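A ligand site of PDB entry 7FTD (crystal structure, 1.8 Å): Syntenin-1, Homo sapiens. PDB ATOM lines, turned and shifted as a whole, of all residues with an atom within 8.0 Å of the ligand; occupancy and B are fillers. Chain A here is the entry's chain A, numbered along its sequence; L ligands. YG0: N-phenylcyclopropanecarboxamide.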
ATOM      1  N   ILE A   5     -20.316  23.505   6.498  1.00  0.00           N
ATOM      2  CA  ILE A   5     -19.990  24.423   7.635  1.00  0.00           C
ATOM      3  C   ILE A   5     -21.229  24.535   8.519  1.00  0.00           C
ATOM      4  O   ILE A   5     -22.180  25.233   8.174  1.00  0.00           O
ATOM      5  CB  ILE A   5     -19.502  25.815   7.172  1.00  0.00           C
ATOM      6  CG1 ILE A   5     -18.721  25.773   5.859  1.00  0.00           C
ATOM      7  CG2 ILE A   5     -18.706  26.503   8.269  1.00  0.00           C
ATOM      8  CD1 ILE A   5     -17.422  25.031   5.960  1.00  0.00           C
ATOM      9  N   ARG A  90     -15.129  25.033  11.232  1.00  0.00           N
ATOM     10  CA  ARG A  90     -14.502  25.683  10.089  1.00  0.00           C
ATOM     11  C   ARG A  90     -15.010  27.098   9.847  1.00  0.00           C
ATOM     12  O   ARG A  90     -15.506  27.389   8.786  1.00  0.00           O
ATOM     13  CB  ARG A  90     -14.755  24.820   8.850  1.00  0.00           C
ATOM     14  CG  ARG A  90     -14.019  23.499   8.934  1.00  0.00           C
ATOM     15  CD  ARG A  90     -14.399  22.537   7.836  1.00  0.00           C
ATOM     16  NE  ARG A  90     -15.727  21.986   8.060  1.00  0.00           N
ATOM     17  CZ  ARG A  90     -16.593  21.699   7.096  1.00  0.00           C
ATOM     18  NH1 ARG A  90     -16.198  21.700   5.837  1.00  0.00           N
ATOM     19  NH2 ARG A  90     -17.833  21.401   7.391  1.00  0.00           N
ATOM     20  N   PRO A  91     -14.787  28.040  10.785  1.00  0.00           N
ATOM     21  CA  PRO A  91     -15.373  29.374  10.711  1.00  0.00           C
ATOM     22  C   PRO A  91     -14.860  30.289   9.600  1.00  0.00           C
ATOM     23  O   PRO A  91     -15.563  31.216   9.202  1.00  0.00           O
ATOM     24  CB  PRO A  91     -14.949  30.067  12.024  1.00  0.00           C
ATOM     25  CG  PRO A  91     -14.297  29.008  12.852  1.00  0.00           C
ATOM     26  CD  PRO A  91     -13.927  27.866  11.958  1.00  0.00           C
ATOM     27  N   PHE A  92     -13.660  29.985   9.073  1.00  0.00           N
ATOM     28  CA  PHE A  92     -13.059  30.742   8.007  1.00  0.00           C
ATOM     29  C   PHE A  92     -13.433  30.118   6.690  1.00  0.00           C
ATOM     30  O   PHE A  92     -12.842  30.453   5.687  1.00  0.00           O
ATOM     31  CB  PHE A  92     -11.524  30.804   8.133  1.00  0.00           C
ATOM     32  CG  PHE A  92     -10.998  31.570   9.324  1.00  0.00           C
ATOM     33  CD1 PHE A  92     -11.511  32.814   9.642  1.00  0.00           C
ATOM     34  CD2 PHE A  92     -10.004  31.038  10.125  1.00  0.00           C
ATOM     35  CE1 PHE A  92     -11.025  33.538  10.721  1.00  0.00           C
ATOM     36  CE2 PHE A  92      -9.510  31.766  11.199  1.00  0.00           C
ATOM     37  CZ  PHE A  92     -10.035  33.009  11.500  1.00  0.00           C
ATOM     38  N   GLU A  93     -14.327  29.136   6.667  1.00  0.00           N
ATOM     39  CA  GLU A  93     -14.600  28.508   5.392  1.00  0.00           C
ATOM     40  C   GLU A  93     -16.049  28.680   4.971  1.00  0.00           C
ATOM     41  O   GLU A  93     -16.929  28.884   5.804  1.00  0.00           O
ATOM     42  CB  GLU A  93     -14.195  27.034   5.456  1.00  0.00           C
ATOM     43  CG  GLU A  93     -12.746  26.893   5.885  1.00  0.00           C
ATOM     44  CD  GLU A  93     -12.252  25.508   6.169  1.00  0.00           C
ATOM     45  OE1 GLU A  93     -12.485  24.611   5.316  1.00  0.00           O
ATOM     46  OE2 GLU A  93     -11.629  25.328   7.256  1.00  0.00           O
ATOM     47  N   ARG A  94     -16.283  28.514   3.669  1.00  0.00           N
ATOM     48  CA  ARG A  94     -17.617  28.418   3.119  1.00  0.00           C
ATOM     49  C   ARG A  94     -17.680  27.259   2.124  1.00  0.00           C
ATOM     50  O   ARG A  94     -16.726  26.978   1.407  1.00  0.00           O
ATOM     51  CB  ARG A  94     -18.047  29.707   2.398  1.00  0.00           C
ATOM     52  CG  ARG A  94     -19.296  29.531   1.550  1.00  0.00           C
ATOM     53  CD  ARG A  94     -19.894  30.826   1.021  1.00  0.00           C
ATOM     54  NE  ARG A  94     -20.139  31.790   2.092  1.00  0.00           N
ATOM     55  CZ  ARG A  94     -21.175  31.774   2.918  1.00  0.00           C
ATOM     56  NH1 ARG A  94     -22.197  30.976   2.683  1.00  0.00           N
ATOM     57  NH2 ARG A  94     -21.211  32.594   3.965  1.00  0.00           N
ATOM     58  N   THR A  95     -18.846  26.638   2.071  1.00  0.00           N
ATOM     59  CA  THR A  95     -19.143  25.570   1.134  1.00  0.00           C
ATOM     60  C   THR A  95     -20.052  26.118   0.061  1.00  0.00           C
ATOM     61  O   THR A  95     -20.959  26.904   0.335  1.00  0.00           O
ATOM     62  CB  THR A  95     -19.790  24.406   1.879  1.00  0.00           C
ATOM     63  OG1 THR A  95     -18.712  23.873   2.662  1.00  0.00           O
ATOM     64  CG2 THR A  95     -20.374  23.340   0.984  1.00  0.00           C
ATOM     65  N   ILE A  96     -19.783  25.692  -1.167  1.00  0.00           N
ATOM     66  CA  ILE A  96     -20.562  26.092  -2.320  1.00  0.00           C
ATOM     67  C   ILE A  96     -20.905  24.810  -3.025  1.00  0.00           C
ATOM     68  O   ILE A  96     -20.000  24.011  -3.237  1.00  0.00           O
ATOM     69  CB  ILE A  96     -19.727  27.001  -3.255  1.00  0.00           C
ATOM     70  CG1 ILE A  96     -19.206  28.256  -2.554  1.00  0.00           C
ATOM     71  CG2 ILE A  96     -20.564  27.321  -4.482  1.00  0.00           C
ATOM     72  CD1 ILE A  96     -20.282  29.259  -2.194  1.00  0.00           C
ATOM     73  N   MET A  98     -22.202  23.123  -6.561  1.00  0.00           N
ATOM     74  CA  MET A  98     -22.289  23.355  -7.987  1.00  0.00           C
ATOM     75  C   MET A  98     -22.890  22.135  -8.712  1.00  0.00           C
ATOM     76  O   MET A  98     -23.094  21.076  -8.120  1.00  0.00           O
ATOM     77  CB  MET A  98     -20.887  23.718  -8.501  1.00  0.00           C
ATOM     78  CG  MET A  98     -20.437  25.142  -8.083  1.00  0.00           C
ATOM     79  SD  MET A  98     -18.649  25.473  -8.198  1.00  0.00           S
ATOM     80  CE  MET A  98     -18.214  25.502  -6.462  1.00  0.00           C
ATOM     81  N   ILE A 115      -8.296  29.132  -6.537  1.00  0.00           N
ATOM     82  CA  ILE A 115      -9.173  29.445  -7.653  1.00  0.00           C
ATOM     83  C   ILE A 115      -8.726  30.795  -8.229  1.00  0.00           C
ATOM     84  O   ILE A 115      -8.293  31.656  -7.454  1.00  0.00           O
ATOM     85  CB  ILE A 115     -10.651  29.438  -7.188  1.00  0.00           C
ATOM     86  CG1 ILE A 115     -11.038  28.146  -6.478  1.00  0.00           C
ATOM     87  CG2 ILE A 115     -11.624  29.709  -8.322  1.00  0.00           C
ATOM     88  CD1 ILE A 115     -12.222  28.287  -5.549  1.00  0.00           C
ATOM     89  N   ALA A 124     -20.368  27.646 -11.395  1.00  0.00           N
ATOM     90  CA  ALA A 124     -19.496  28.412 -10.510  1.00  0.00           C
ATOM     91  C   ALA A 124     -19.854  29.900 -10.534  1.00  0.00           C
ATOM     92  O   ALA A 124     -19.884  30.577  -9.488  1.00  0.00           O
ATOM     93  CB  ALA A 124     -18.072  28.181 -10.927  1.00  0.00           C
ATOM     94  N   ASN A 127     -23.343  30.382  -9.074  1.00  0.00           N
ATOM     95  CA  ASN A 127     -23.290  30.132  -7.635  1.00  0.00           C
ATOM     96  C   ASN A 127     -22.428  31.159  -6.903  1.00  0.00           C
ATOM     97  O   ASN A 127     -22.430  31.218  -5.677  1.00  0.00           O
ATOM     98  CB  ASN A 127     -22.921  28.663  -7.346  1.00  0.00           C
ATOM     99  CG  ASN A 127     -24.150  27.781  -7.367  1.00  0.00           C
ATOM    100  OD1 ASN A 127     -24.813  27.646  -6.350  1.00  0.00           O
ATOM    101  ND2 ASN A 127     -24.524  27.250  -8.526  1.00  0.00           N
ATOM    102  N   GLY A 128     -21.715  32.024  -7.623  1.00  0.00           N
ATOM    103  CA  GLY A 128     -20.975  33.105  -6.997  1.00  0.00           C
ATOM    104  C   GLY A 128     -19.678  32.658  -6.353  1.00  0.00           C
ATOM    105  O   GLY A 128     -19.285  33.135  -5.271  1.00  0.00           O
ATOM    106  N   LEU A 129     -19.013  31.714  -7.028  1.00  0.00           N
ATOM    107  CA  LEU A 129     -17.714  31.253  -6.586  1.00  0.00           C
ATOM    108  C   LEU A 129     -16.703  32.390  -6.728  1.00  0.00           C
ATOM    109  O   LEU A 129     -16.750  33.192  -7.643  1.00  0.00           O
ATOM    110  CB  LEU A 129     -17.290  30.014  -7.373  1.00  0.00           C
ATOM    111  CG  LEU A 129     -16.007  29.331  -6.874  1.00  0.00           C
ATOM    112  CD1 LEU A 129     -16.225  28.678  -5.528  1.00  0.00           C
ATOM    113  CD2 LEU A 129     -15.527  28.298  -7.886  1.00  0.00           C
ATOM    114  N   LEU A 130     -15.767  32.458  -5.797  1.00  0.00           N
ATOM    115  CA  LEU A 130     -14.826  33.544  -5.792  1.00  0.00           C
ATOM    116  C   LEU A 130     -13.426  33.001  -6.052  1.00  0.00           C
ATOM    117  O   LEU A 130     -13.085  31.909  -5.630  1.00  0.00           O
ATOM    118  CB  LEU A 130     -14.876  34.226  -4.422  1.00  0.00           C
ATOM    119  CG  LEU A 130     -16.255  34.753  -4.031  1.00  0.00           C
ATOM    120  CD1 LEU A 130     -16.185  35.382  -2.673  1.00  0.00           C
ATOM    121  CD2 LEU A 130     -16.813  35.753  -5.068  1.00  0.00           C
ATOM    122  N   THR A 131     -12.620  33.884  -6.643  1.00  0.00           N
ATOM    123  CA  THR A 131     -11.209  33.647  -6.835  1.00  0.00           C
ATOM    124  C   THR A 131     -10.488  34.064  -5.577  1.00  0.00           C
ATOM    125  O   THR A 131     -11.132  34.562  -4.641  1.00  0.00           O
ATOM    126  CB  THR A 131     -10.733  34.453  -8.054  1.00  0.00           C
ATOM    127  OG1 THR A 131     -10.959  35.825  -7.744  1.00  0.00           O
ATOM    128  CG2 THR A 131     -11.483  34.124  -9.315  1.00  0.00           C
ATOM    129  N   GLU A 132      -9.174  33.851  -5.554  1.00  0.00           N
ATOM    130  CA  GLU A 132      -8.332  34.155  -4.397  1.00  0.00           C
ATOM    131  C   GLU A 132      -8.868  33.399  -3.181  1.00  0.00           C
ATOM    132  O   GLU A 132      -8.737  33.840  -2.035  1.00  0.00           O
ATOM    133  CB  GLU A 132      -8.283  35.677  -4.245  1.00  0.00           C
ATOM    134  CG  GLU A 132      -7.177  36.188  -3.329  1.00  0.00           C
ATOM    135  CD  GLU A 132      -5.778  36.031  -3.892  1.00  0.00           C
ATOM    136  OE1 GLU A 132      -5.652  35.544  -5.045  1.00  0.00           O
ATOM    137  OE2 GLU A 132      -4.822  36.372  -3.160  1.00  0.00           O
ATOM    138  N   HIS A 133      -9.435  32.224  -3.431  1.00  0.00           N
ATOM    139  CA  HIS A 133      -9.854  31.309  -2.381  1.00  0.00           C
ATOM    140  C   HIS A 133      -9.140  29.967  -2.579  1.00  0.00           C
ATOM    141  O   HIS A 133      -9.078  29.427  -3.673  1.00  0.00           O
ATOM    142  CB  HIS A 133     -11.388  31.173  -2.416  1.00  0.00           C
ATOM    143  CG  HIS A 133     -12.151  32.274  -1.743  1.00  0.00           C
ATOM    144  ND1 HIS A 133     -12.045  33.594  -2.072  1.00  0.00           N
ATOM    145  CD2 HIS A 133     -13.097  32.232  -0.793  1.00  0.00           C
ATOM    146  CE1 HIS A 133     -12.870  34.327  -1.342  1.00  0.00           C
ATOM    147  NE2 HIS A 133     -13.528  33.523  -0.569  1.00  0.00           N
ATOM    148  N   ILE A 164     -17.846  22.156  -2.685  1.00  0.00           N
ATOM    149  CA  ILE A 164     -16.498  22.616  -2.457  1.00  0.00           C
ATOM    150  C   ILE A 164     -16.466  23.521  -1.224  1.00  0.00           C
ATOM    151  O   ILE A 164     -17.278  24.433  -1.072  1.00  0.00           O
ATOM    152  CB  ILE A 164     -15.967  23.323  -3.724  1.00  0.00           C
ATOM    153  CG1 ILE A 164     -16.161  22.432  -4.962  1.00  0.00           C
ATOM    154  CG2 ILE A 164     -14.520  23.742  -3.567  1.00  0.00           C
ATOM    155  CD1 ILE A 164     -15.750  23.089  -6.265  1.00  0.00           C
ATOM    156  N   THR A 165     -15.522  23.240  -0.333  1.00  0.00           N
ATOM    157  CA  THR A 165     -15.241  24.105   0.791  1.00  0.00           C
ATOM    158  C   THR A 165     -13.942  24.882   0.550  1.00  0.00           C
ATOM    159  O   THR A 165     -12.919  24.270   0.242  1.00  0.00           O
ATOM    160  CB  THR A 165     -15.097  23.290   2.064  1.00  0.00           C
ATOM    161  OG1 THR A 165     -16.383  22.730   2.261  1.00  0.00           O
ATOM    162  CG2 THR A 165     -14.629  24.110   3.239  1.00  0.00           C
ATOM    163  N   ILE A 166     -14.001  26.203   0.782  1.00  0.00           N
ATOM    164  CA  ILE A 166     -13.013  27.164   0.340  1.00  0.00           C
ATOM    165  C   ILE A 166     -12.746  28.158   1.460  1.00  0.00           C
ATOM    166  O   ILE A 166     -13.641  28.466   2.244  1.00  0.00           O
ATOM    167  CB  ILE A 166     -13.507  27.852  -0.956  1.00  0.00           C
ATOM    168  CG1 ILE A 166     -14.758  28.691  -0.752  1.00  0.00           C
ATOM    169  CG2 ILE A 166     -13.730  26.801  -2.026  1.00  0.00           C
ATOM    170  CD1 ILE A 166     -15.395  29.152  -2.039  1.00  0.00           C
ATOM    171  N   MET A 167     -11.496  28.634   1.486  1.00  0.00           N
ATOM    172  CA  MET A 167     -11.015  29.537   2.501  1.00  0.00           C
ATOM    173  C   MET A 167     -10.324  30.702   1.799  1.00  0.00           C
ATOM    174  O   MET A 167      -9.642  30.529   0.792  1.00  0.00           O
ATOM    175  CB  MET A 167     -10.031  28.846   3.458  1.00  0.00           C
ATOM    176  CG  MET A 167      -9.563  29.776   4.478  1.00  0.00           C
ATOM    177  SD  MET A 167      -8.370  29.059   5.553  1.00  0.00           S
ATOM    178  CE  MET A 167      -9.298  27.682   6.240  1.00  0.00           C
ATOM    179  N   PRO A 168     -10.513  31.964   2.240  1.00  0.00           N
ATOM    180  CA  PRO A 168      -9.814  33.076   1.599  1.00  0.00           C
ATOM    181  C   PRO A 168      -8.308  32.858   1.654  1.00  0.00           C
ATOM    182  O   PRO A 168      -7.774  32.736   2.744  1.00  0.00           O
ATOM    183  CB  PRO A 168     -10.255  34.319   2.384  1.00  0.00           C
ATOM    184  CG  PRO A 168     -11.609  33.906   2.980  1.00  0.00           C
ATOM    185  CD  PRO A 168     -11.473  32.420   3.254  1.00  0.00           C
ATOM    186  N   ILE A 171      -6.146  33.981   4.547  1.00  0.00           N
ATOM    187  CA  ILE A 171      -6.312  33.251   5.784  1.00  0.00           C
ATOM    188  C   ILE A 171      -5.669  31.873   5.648  1.00  0.00           C
ATOM    189  O   ILE A 171      -4.965  31.410   6.546  1.00  0.00           O
ATOM    190  CB  ILE A 171      -7.792  33.154   6.188  1.00  0.00           C
ATOM    191  CG1 ILE A 171      -8.424  34.559   6.267  1.00  0.00           C
ATOM    192  CG2 ILE A 171      -7.918  32.385   7.487  1.00  0.00           C
ATOM    193  CD1 ILE A 171      -9.821  34.576   6.749  1.00  0.00           C
HETATM  194  C4  YG0 L   1     -18.737  32.624  -1.914  1.00  0.00           C
HETATM  195  C5  YG0 L   1     -19.034  33.403  -0.826  1.00  0.00           C
HETATM  196  C6  YG0 L   1     -18.103  33.571   0.205  1.00  0.00           C
HETATM  197  C7  YG0 L   1     -15.175  33.568   3.466  1.00  0.00           C
HETATM  198  C8  YG0 L   1     -15.589  34.154   4.782  1.00  0.00           C
HETATM  199  O   YG0 L   1     -17.353  32.697   2.933  1.00  0.00           O
HETATM  200  C   YG0 L   1     -16.256  33.109   2.515  1.00  0.00           C
HETATM  201  C9  YG0 L   1     -15.011  32.794   4.745  1.00  0.00           C
HETATM  202  N   YG0 L   1     -15.948  33.236   1.204  1.00  0.00           N
HETATM  203  C1  YG0 L   1     -16.853  32.975   0.131  1.00  0.00           C
HETATM  204  C3  YG0 L   1     -17.497  32.014  -1.992  1.00  0.00           C
HETATM  205  C2  YG0 L   1     -16.552  32.182  -0.982  1.00  0.00           C
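A ring nitrogen (NE2) of His 133 lies within hydrogen-bond range of a nitrogen (N) of the ligand (3.0 Å).
The guanidinium group of Arg 94 is in hydrogen-bond range of an oxygen (O) of the ligand, at 3.0 Å.
A ring nitrogen (ND1) of His 133 is in hydrogen-bond range of the backbone carbonyl oxygen of Thr 131 (2.9 Å).
The backbone NH (N) of Ile 115 lies within hydrogen-bond range of the backbone carbonyl oxygen (O) of His 133 (3.0 Å).
N of Ile 166 is in hydrogen-bond range of O of Arg 94 (2.9 Å).
The backbone NH (N) of Ile 96 is in hydrogen-bond range of the backbone carbonyl oxygen (O) of Ile 164 (2.8 Å).
Phe 92 touches the ligand.
Ile 96 touches the ligand (CD1 to C4, 3.7 Å).
Gly 128 touches the ligand (O to C4, 3.4 Å).
Leu 130 touches the ligand.
Ile 166 touches the ligand (CD1 to C2, 3.4 Å).
CG of Pro 168 touches C7 of the ligand (3.6 Å).
Within 4 Å of the ligand: Phe 92, Arg 94, Ile 96, Gly 128, Leu 130, His 133, Ile 166 and Pro 168.
The nearest printed residue that does not touch the ligand is Glu 93 (4.2 Å).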
